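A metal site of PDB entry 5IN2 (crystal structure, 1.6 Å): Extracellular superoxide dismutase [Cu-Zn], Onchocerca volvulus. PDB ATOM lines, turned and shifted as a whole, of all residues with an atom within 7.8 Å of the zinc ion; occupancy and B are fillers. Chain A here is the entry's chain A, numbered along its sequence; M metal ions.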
ATOM      1  N   PHE A  45     -18.350   3.982 -13.829  1.00  0.00           N
ATOM      2  CA  PHE A  45     -18.446   3.535 -12.433  1.00  0.00           C
ATOM      3  C   PHE A  45     -19.847   3.814 -11.962  1.00  0.00           C
ATOM      4  O   PHE A  45     -20.245   4.974 -11.877  1.00  0.00           O
ATOM      5  CB  PHE A  45     -17.397   4.297 -11.642  1.00  0.00           C
ATOM      6  CG  PHE A  45     -17.086   3.760 -10.261  1.00  0.00           C
ATOM      7  CD1 PHE A  45     -16.636   2.476 -10.091  1.00  0.00           C
ATOM      8  CD2 PHE A  45     -17.094   4.614  -9.171  1.00  0.00           C
ATOM      9  CE1 PHE A  45     -16.262   2.025  -8.822  1.00  0.00           C
ATOM     10  CE2 PHE A  45     -16.727   4.169  -7.919  1.00  0.00           C
ATOM     11  CZ  PHE A  45     -16.316   2.864  -7.762  1.00  0.00           C
ATOM     12  N   HIS A  46     -20.645   2.783 -11.719  1.00  0.00           N
ATOM     13  CA  HIS A  46     -22.049   2.967 -11.405  1.00  0.00           C
ATOM     14  C   HIS A  46     -22.544   2.031 -10.334  1.00  0.00           C
ATOM     15  O   HIS A  46     -22.104   0.907 -10.260  1.00  0.00           O
ATOM     16  CB  HIS A  46     -22.960   2.710 -12.597  1.00  0.00           C
ATOM     17  CG  HIS A  46     -22.470   3.238 -13.912  1.00  0.00           C
ATOM     18  ND1 HIS A  46     -22.323   2.412 -15.004  1.00  0.00           N
ATOM     19  CD2 HIS A  46     -22.163   4.498 -14.324  1.00  0.00           C
ATOM     20  CE1 HIS A  46     -21.896   3.133 -16.031  1.00  0.00           C
ATOM     21  NE2 HIS A  46     -21.800   4.391 -15.655  1.00  0.00           N
ATOM     22  N   VAL A  47     -23.485   2.514  -9.541  1.00  0.00           N
ATOM     23  CA  VAL A  47     -24.326   1.619  -8.735  1.00  0.00           C
ATOM     24  C   VAL A  47     -25.505   1.169  -9.601  1.00  0.00           C
ATOM     25  O   VAL A  47     -26.261   1.990 -10.145  1.00  0.00           O
ATOM     26  CB  VAL A  47     -24.832   2.296  -7.457  1.00  0.00           C
ATOM     27  CG1 VAL A  47     -25.703   1.323  -6.639  1.00  0.00           C
ATOM     28  CG2 VAL A  47     -23.705   2.788  -6.615  1.00  0.00           C
ATOM     29  N   HIS A  48     -25.661  -0.147  -9.737  1.00  0.00           N
ATOM     30  CA  HIS A  48     -26.712  -0.727 -10.545  1.00  0.00           C
ATOM     31  C   HIS A  48     -27.869  -1.152  -9.676  1.00  0.00           C
ATOM     32  O   HIS A  48     -27.736  -1.172  -8.449  1.00  0.00           O
ATOM     33  CB  HIS A  48     -26.146  -1.901 -11.373  1.00  0.00           C
ATOM     34  CG  HIS A  48     -25.401  -1.462 -12.600  1.00  0.00           C
ATOM     35  ND1 HIS A  48     -25.799  -1.808 -13.871  1.00  0.00           N
ATOM     36  CD2 HIS A  48     -24.299  -0.691 -12.745  1.00  0.00           C
ATOM     37  CE1 HIS A  48     -24.963  -1.289 -14.756  1.00  0.00           C
ATOM     38  NE2 HIS A  48     -24.048  -0.603 -14.100  1.00  0.00           N
ATOM     39  N   ASP A  62     -29.964  -2.509 -14.743  1.00  0.00           N
ATOM     40  CA  ASP A  62     -29.593  -1.174 -15.203  1.00  0.00           C
ATOM     41  C   ASP A  62     -29.098  -0.291 -14.065  1.00  0.00           C
ATOM     42  O   ASP A  62     -28.825  -0.758 -12.983  1.00  0.00           O
ATOM     43  CB  ASP A  62     -30.789  -0.554 -15.900  1.00  0.00           C
ATOM     44  CG  ASP A  62     -31.247  -1.366 -17.098  1.00  0.00           C
ATOM     45  OD1 ASP A  62     -30.367  -1.913 -17.808  1.00  0.00           O
ATOM     46  OD2 ASP A  62     -32.468  -1.483 -17.292  1.00  0.00           O
ATOM     47  N   HIS A  63     -28.898   0.999 -14.317  1.00  0.00           N
ATOM     48  CA  HIS A  63     -28.385   1.851 -13.250  1.00  0.00           C
ATOM     49  C   HIS A  63     -29.444   2.053 -12.191  1.00  0.00           C
ATOM     50  O   HIS A  63     -30.623   2.143 -12.509  1.00  0.00           O
ATOM     51  CB  HIS A  63     -27.963   3.205 -13.792  1.00  0.00           C
ATOM     52  CG  HIS A  63     -26.855   3.120 -14.793  1.00  0.00           C
ATOM     53  ND1 HIS A  63     -26.262   4.229 -15.357  1.00  0.00           N
ATOM     54  CD2 HIS A  63     -26.226   2.049 -15.331  1.00  0.00           C
ATOM     55  CE1 HIS A  63     -25.326   3.851 -16.208  1.00  0.00           C
ATOM     56  NE2 HIS A  63     -25.275   2.526 -16.206  1.00  0.00           N
ATOM     57  N   TYR A  64     -29.012   2.201 -10.944  1.00  0.00           N
ATOM     58  CA  TYR A  64     -29.924   2.504  -9.858  1.00  0.00           C
ATOM     59  C   TYR A  64     -30.506   3.908 -10.076  1.00  0.00           C
ATOM     60  O   TYR A  64     -29.766   4.892 -10.089  1.00  0.00           O
ATOM     61  CB  TYR A  64     -29.211   2.399  -8.512  1.00  0.00           C
ATOM     62  CG  TYR A  64     -30.094   2.643  -7.320  1.00  0.00           C
ATOM     63  CD1 TYR A  64     -31.349   2.098  -7.265  1.00  0.00           C
ATOM     64  CD2 TYR A  64     -29.648   3.433  -6.278  1.00  0.00           C
ATOM     65  CE1 TYR A  64     -32.182   2.336  -6.172  1.00  0.00           C
ATOM     66  CE2 TYR A  64     -30.478   3.669  -5.175  1.00  0.00           C
ATOM     67  CZ  TYR A  64     -31.732   3.096  -5.150  1.00  0.00           C
ATOM     68  OH  TYR A  64     -32.588   3.312  -4.087  1.00  0.00           O
ATOM     69  N   ASN A  65     -31.837   3.961 -10.214  1.00  0.00           N
ATOM     70  CA  ASN A  65     -32.509   5.170 -10.685  1.00  0.00           C
ATOM     71  C   ASN A  65     -33.904   5.333 -10.070  1.00  0.00           C
ATOM     72  O   ASN A  65     -34.904   5.323 -10.806  1.00  0.00           O
ATOM     73  CB  ASN A  65     -32.595   5.102 -12.186  1.00  0.00           C
ATOM     74  CG  ASN A  65     -33.159   6.345 -12.810  1.00  0.00           C
ATOM     75  OD1 ASN A  65     -33.041   7.437 -12.266  1.00  0.00           O
ATOM     76  ND2 ASN A  65     -33.727   6.182 -13.975  1.00  0.00           N
ATOM     77  N   LYS A  69     -34.868   9.298 -13.695  1.00  0.00           N
ATOM     78  CA  LYS A  69     -34.233  10.351 -14.489  1.00  0.00           C
ATOM     79  C   LYS A  69     -33.376   9.754 -15.614  1.00  0.00           C
ATOM     80  O   LYS A  69     -33.220   8.546 -15.719  1.00  0.00           O
ATOM     81  CB  LYS A  69     -33.359  11.235 -13.608  1.00  0.00           C
ATOM     82  CG  LYS A  69     -34.065  11.814 -12.380  1.00  0.00           C
ATOM     83  CD  LYS A  69     -35.213  12.678 -12.796  1.00  0.00           C
ATOM     84  CE  LYS A  69     -35.701  13.529 -11.633  1.00  0.00           C
ATOM     85  NZ  LYS A  69     -37.052  14.087 -11.911  1.00  0.00           N
ATOM     86  N   THR A  70     -32.841  10.627 -16.463  1.00  0.00           N
ATOM     87  CA  THR A  70     -31.877  10.221 -17.465  1.00  0.00           C
ATOM     88  C   THR A  70     -30.489  10.113 -16.856  1.00  0.00           C
ATOM     89  O   THR A  70     -30.194  10.665 -15.799  1.00  0.00           O
ATOM     90  CB  THR A  70     -31.831  11.185 -18.644  1.00  0.00           C
ATOM     91  OG1 THR A  70     -31.740  12.517 -18.145  1.00  0.00           O
ATOM     92  CG2 THR A  70     -33.078  11.010 -19.507  1.00  0.00           C
ATOM     93  N   HIS A  71     -29.632   9.391 -17.550  1.00  0.00           N
ATOM     94  CA  HIS A  71     -28.252   9.230 -17.162  1.00  0.00           C
ATOM     95  C   HIS A  71     -27.496  10.550 -17.210  1.00  0.00           C
ATOM     96  O   HIS A  71     -27.706  11.346 -18.127  1.00  0.00           O
ATOM     97  CB  HIS A  71     -27.577   8.222 -18.087  1.00  0.00           C
ATOM     98  CG  HIS A  71     -26.167   7.943 -17.721  1.00  0.00           C
ATOM     99  ND1 HIS A  71     -25.805   7.184 -16.631  1.00  0.00           N
ATOM    100  CD2 HIS A  71     -25.007   8.325 -18.315  1.00  0.00           C
ATOM    101  CE1 HIS A  71     -24.485   7.150 -16.539  1.00  0.00           C
ATOM    102  NE2 HIS A  71     -23.977   7.844 -17.561  1.00  0.00           N
ATOM    103  N   GLY A  72     -26.628  10.781 -16.241  1.00  0.00           N
ATOM    104  CA  GLY A  72     -25.724  11.916 -16.242  1.00  0.00           C
ATOM    105  C   GLY A  72     -24.445  11.631 -15.496  1.00  0.00           C
ATOM    106  O   GLY A  72     -24.099  10.475 -15.272  1.00  0.00           O
ATOM    107  N   GLY A  73     -23.740  12.697 -15.162  1.00  0.00           N
ATOM    108  CA  GLY A  73     -22.568  12.597 -14.302  1.00  0.00           C
ATOM    109  C   GLY A  73     -22.923  12.844 -12.869  1.00  0.00           C
ATOM    110  O   GLY A  73     -23.972  13.383 -12.561  1.00  0.00           O
ATOM    111  N   LYS A  79     -29.673  13.084 -12.998  1.00  0.00           N
ATOM    112  CA  LYS A  79     -28.825  11.924 -13.179  1.00  0.00           C
ATOM    113  C   LYS A  79     -29.534  10.733 -12.549  1.00  0.00           C
ATOM    114  O   LYS A  79     -30.526  10.904 -11.856  1.00  0.00           O
ATOM    115  CB  LYS A  79     -27.470  12.131 -12.514  1.00  0.00           C
ATOM    116  CG  LYS A  79     -27.558  12.394 -11.025  1.00  0.00           C
ATOM    117  CD  LYS A  79     -26.194  12.310 -10.322  1.00  0.00           C
ATOM    118  CE  LYS A  79     -26.388  12.697  -8.891  1.00  0.00           C
ATOM    119  NZ  LYS A  79     -25.196  12.578  -8.043  1.00  0.00           N
ATOM    120  N   HIS A  80     -29.012   9.529 -12.772  1.00  0.00           N
ATOM    121  CA  HIS A  80     -29.363   8.400 -11.931  1.00  0.00           C
ATOM    122  C   HIS A  80     -28.649   8.527 -10.600  1.00  0.00           C
ATOM    123  O   HIS A  80     -27.501   8.932 -10.542  1.00  0.00           O
ATOM    124  CB  HIS A  80     -28.975   7.094 -12.607  1.00  0.00           C
ATOM    125  CG  HIS A  80     -29.530   6.912 -13.981  1.00  0.00           C
ATOM    126  ND1 HIS A  80     -28.821   6.300 -14.997  1.00  0.00           N
ATOM    127  CD2 HIS A  80     -30.743   7.229 -14.501  1.00  0.00           C
ATOM    128  CE1 HIS A  80     -29.590   6.228 -16.071  1.00  0.00           C
ATOM    129  NE2 HIS A  80     -30.740   6.811 -15.801  1.00  0.00           N
ATOM    130  N   ILE A  81     -29.308   8.168  -9.506  1.00  0.00           N
ATOM    131  CA  ILE A  81     -28.615   8.154  -8.227  1.00  0.00           C
ATOM    132  C   ILE A  81     -27.312   7.364  -8.270  1.00  0.00           C
ATOM    133  O   ILE A  81     -26.305   7.764  -7.684  1.00  0.00           O
ATOM    134  CB  ILE A  81     -29.522   7.599  -7.102  1.00  0.00           C
ATOM    135  CG1 ILE A  81     -30.649   8.578  -6.797  1.00  0.00           C
ATOM    136  CG2 ILE A  81     -28.707   7.291  -5.830  1.00  0.00           C
ATOM    137  CD1 ILE A  81     -30.191   9.911  -6.197  1.00  0.00           C
ATOM    138  N   GLY A  82     -27.305   6.241  -8.992  1.00  0.00           N
ATOM    139  CA  GLY A  82     -26.133   5.401  -9.088  1.00  0.00           C
ATOM    140  C   GLY A  82     -25.006   5.888  -9.973  1.00  0.00           C
ATOM    141  O   GLY A  82     -23.988   5.212 -10.119  1.00  0.00           O
ATOM    142  N   ASP A  83     -25.153   7.061 -10.577  1.00  0.00           N
ATOM    143  CA  ASP A  83     -24.172   7.549 -11.538  1.00  0.00           C
ATOM    144  C   ASP A  83     -22.959   8.134 -10.825  1.00  0.00           C
ATOM    145  O   ASP A  83     -23.047   9.191 -10.212  1.00  0.00           O
ATOM    146  CB  ASP A  83     -24.790   8.617 -12.455  1.00  0.00           C
ATOM    147  CG  ASP A  83     -25.751   8.047 -13.438  1.00  0.00           C
ATOM    148  OD1 ASP A  83     -25.732   6.814 -13.731  1.00  0.00           O
ATOM    149  OD2 ASP A  83     -26.569   8.815 -13.985  1.00  0.00           O
ATOM    150  N   LEU A  84     -21.814   7.460 -10.909  1.00  0.00           N
ATOM    151  CA  LEU A  84     -20.619   7.916 -10.235  1.00  0.00           C
ATOM    152  C   LEU A  84     -19.501   8.290 -11.215  1.00  0.00           C
ATOM    153  O   LEU A  84     -18.351   8.435 -10.820  1.00  0.00           O
ATOM    154  CB  LEU A  84     -20.132   6.855  -9.233  1.00  0.00           C
ATOM    155  CG  LEU A  84     -21.069   6.625  -8.041  1.00  0.00           C
ATOM    156  CD1 LEU A  84     -20.541   5.459  -7.227  1.00  0.00           C
ATOM    157  CD2 LEU A  84     -21.194   7.892  -7.167  1.00  0.00           C
ATOM    158  N   GLY A  85     -19.861   8.497 -12.479  1.00  0.00           N
ATOM    159  CA  GLY A  85     -18.884   9.001 -13.445  1.00  0.00           C
ATOM    160  C   GLY A  85     -17.818   8.016 -13.839  1.00  0.00           C
ATOM    161  O   GLY A  85     -18.105   6.841 -14.120  1.00  0.00           O
ATOM    162  N   ASP A 124     -17.478   6.536 -19.466  1.00  0.00           N
ATOM    163  CA  ASP A 124     -18.852   7.011 -19.339  1.00  0.00           C
ATOM    164  C   ASP A 124     -18.899   8.427 -19.904  1.00  0.00           C
ATOM    165  O   ASP A 124     -18.202   9.299 -19.389  1.00  0.00           O
ATOM    166  CB  ASP A 124     -19.242   6.978 -17.860  1.00  0.00           C
ATOM    167  CG  ASP A 124     -20.674   7.352 -17.571  1.00  0.00           C
ATOM    168  OD1 ASP A 124     -21.336   8.047 -18.375  1.00  0.00           O
ATOM    169  OD2 ASP A 124     -21.144   6.955 -16.472  1.00  0.00           O
ATOM    170  N   GLY A 127     -23.793  11.175 -20.241  1.00  0.00           N
ATOM    171  CA  GLY A 127     -25.051  11.617 -20.819  1.00  0.00           C
ATOM    172  C   GLY A 127     -24.854  12.735 -21.848  1.00  0.00           C
ATOM    173  O   GLY A 127     -25.835  13.424 -22.222  1.00  0.00           O
ATOM    174  N   SER A 137     -26.410   6.970 -24.611  1.00  0.00           N
ATOM    175  CA  SER A 137     -25.776   7.887 -23.650  1.00  0.00           C
ATOM    176  C   SER A 137     -26.703   8.205 -22.465  1.00  0.00           C
ATOM    177  O   SER A 137     -26.261   8.199 -21.320  1.00  0.00           O
ATOM    178  CB  SER A 137     -25.356   9.197 -24.346  1.00  0.00           C
ATOM    179  OG  SER A 137     -24.823  10.131 -23.430  1.00  0.00           O
ATOM    180  N   LEU A 138     -27.967   8.496 -22.751  1.00  0.00           N
ATOM    181  CA  LEU A 138     -28.904   8.908 -21.713  1.00  0.00           C
ATOM    182  C   LEU A 138     -29.433   7.730 -20.928  1.00  0.00           C
ATOM    183  O   LEU A 138     -30.191   7.926 -19.985  1.00  0.00           O
ATOM    184  CB  LEU A 138     -30.065   9.671 -22.340  1.00  0.00           C
ATOM    185  CG  LEU A 138     -29.719  11.019 -22.975  1.00  0.00           C
ATOM    186  CD1 LEU A 138     -30.937  11.540 -23.690  1.00  0.00           C
ATOM    187  CD2 LEU A 138     -29.264  11.971 -21.903  1.00  0.00           C
ATOM    188  N   LYS A 139     -29.052   6.531 -21.316  1.00  0.00           N
ATOM    189  CA  LYS A 139     -29.390   5.324 -20.557  1.00  0.00           C
ATOM    190  C   LYS A 139     -28.212   4.843 -19.704  1.00  0.00           C
ATOM    191  O   LYS A 139     -28.351   4.604 -18.500  1.00  0.00           O
ATOM    192  CB  LYS A 139     -29.818   4.212 -21.507  1.00  0.00           C
ATOM    193  CG  LYS A 139     -31.131   4.449 -22.220  1.00  0.00           C
ATOM    194  CD  LYS A 139     -31.403   3.335 -23.241  1.00  0.00           C
ATOM    195  CE  LYS A 139     -32.629   3.610 -24.100  1.00  0.00           C
ATOM    196  NZ  LYS A 139     -32.838   2.523 -25.104  1.00  0.00           N
ATOM    197  N   THR A 140     -27.057   4.682 -20.336  1.00  0.00           N
ATOM    198  CA  THR A 140     -25.904   4.044 -19.683  1.00  0.00           C
ATOM    199  C   THR A 140     -24.595   4.817 -19.729  1.00  0.00           C
ATOM    200  O   THR A 140     -23.628   4.408 -19.129  1.00  0.00           O
ATOM    201  CB  THR A 140     -25.584   2.678 -20.315  1.00  0.00           C
ATOM    202  OG1 THR A 140     -25.144   2.897 -21.663  1.00  0.00           O
ATOM    203  CG2 THR A 140     -26.801   1.777 -20.295  1.00  0.00           C
ATOM    204  N   GLY A 141     -24.539   5.893 -20.505  1.00  0.00           N
ATOM    205  CA  GLY A 141     -23.283   6.588 -20.696  1.00  0.00           C
ATOM    206  C   GLY A 141     -22.312   5.917 -21.674  1.00  0.00           C
ATOM    207  O   GLY A 141     -21.171   6.320 -21.813  1.00  0.00           O
HETATM  208 ZN    ZN M   1     -26.775   6.163 -15.158  1.00  0.00          ZN
HETATM  209 CU    CU M   2     -22.972   0.465 -15.469  1.00  0.00          CU
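The side-chain carboxylate (OD2) of Asp 83 is in hydrogen-bond range of the backbone NH (N) of Gly 72 (3.0 Å).
A ring nitrogen (NE2) of His 63 lies close to a ring nitrogen (ND1) of His 46.
OD1 of Asp 124 is in hydrogen-bond range of NE2 of His 71, at 2.8 Å.
The backbone NH of His 71 sits at hydrogen-bond distance from the backbone carbonyl oxygen of Leu 138.
The backbone carbonyl oxygen (O) of Thr 70 sits at hydrogen-bond distance from the backbone NH (N) of His 80, 3.4 Å away.
NE2 of His 80 lies within hydrogen-bond range of O of Lys 69 (3.0 Å).
The zinc ion is bound by the side-chain carboxylate (OD1) of Asp 83 (1.9 Å), a ring nitrogen (ND1) of His 63 (2.0 Å), a ring nitrogen (ND1) of His 71 (2.0 Å) and a ring nitrogen (ND1) of His 80 (2.1 Å).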
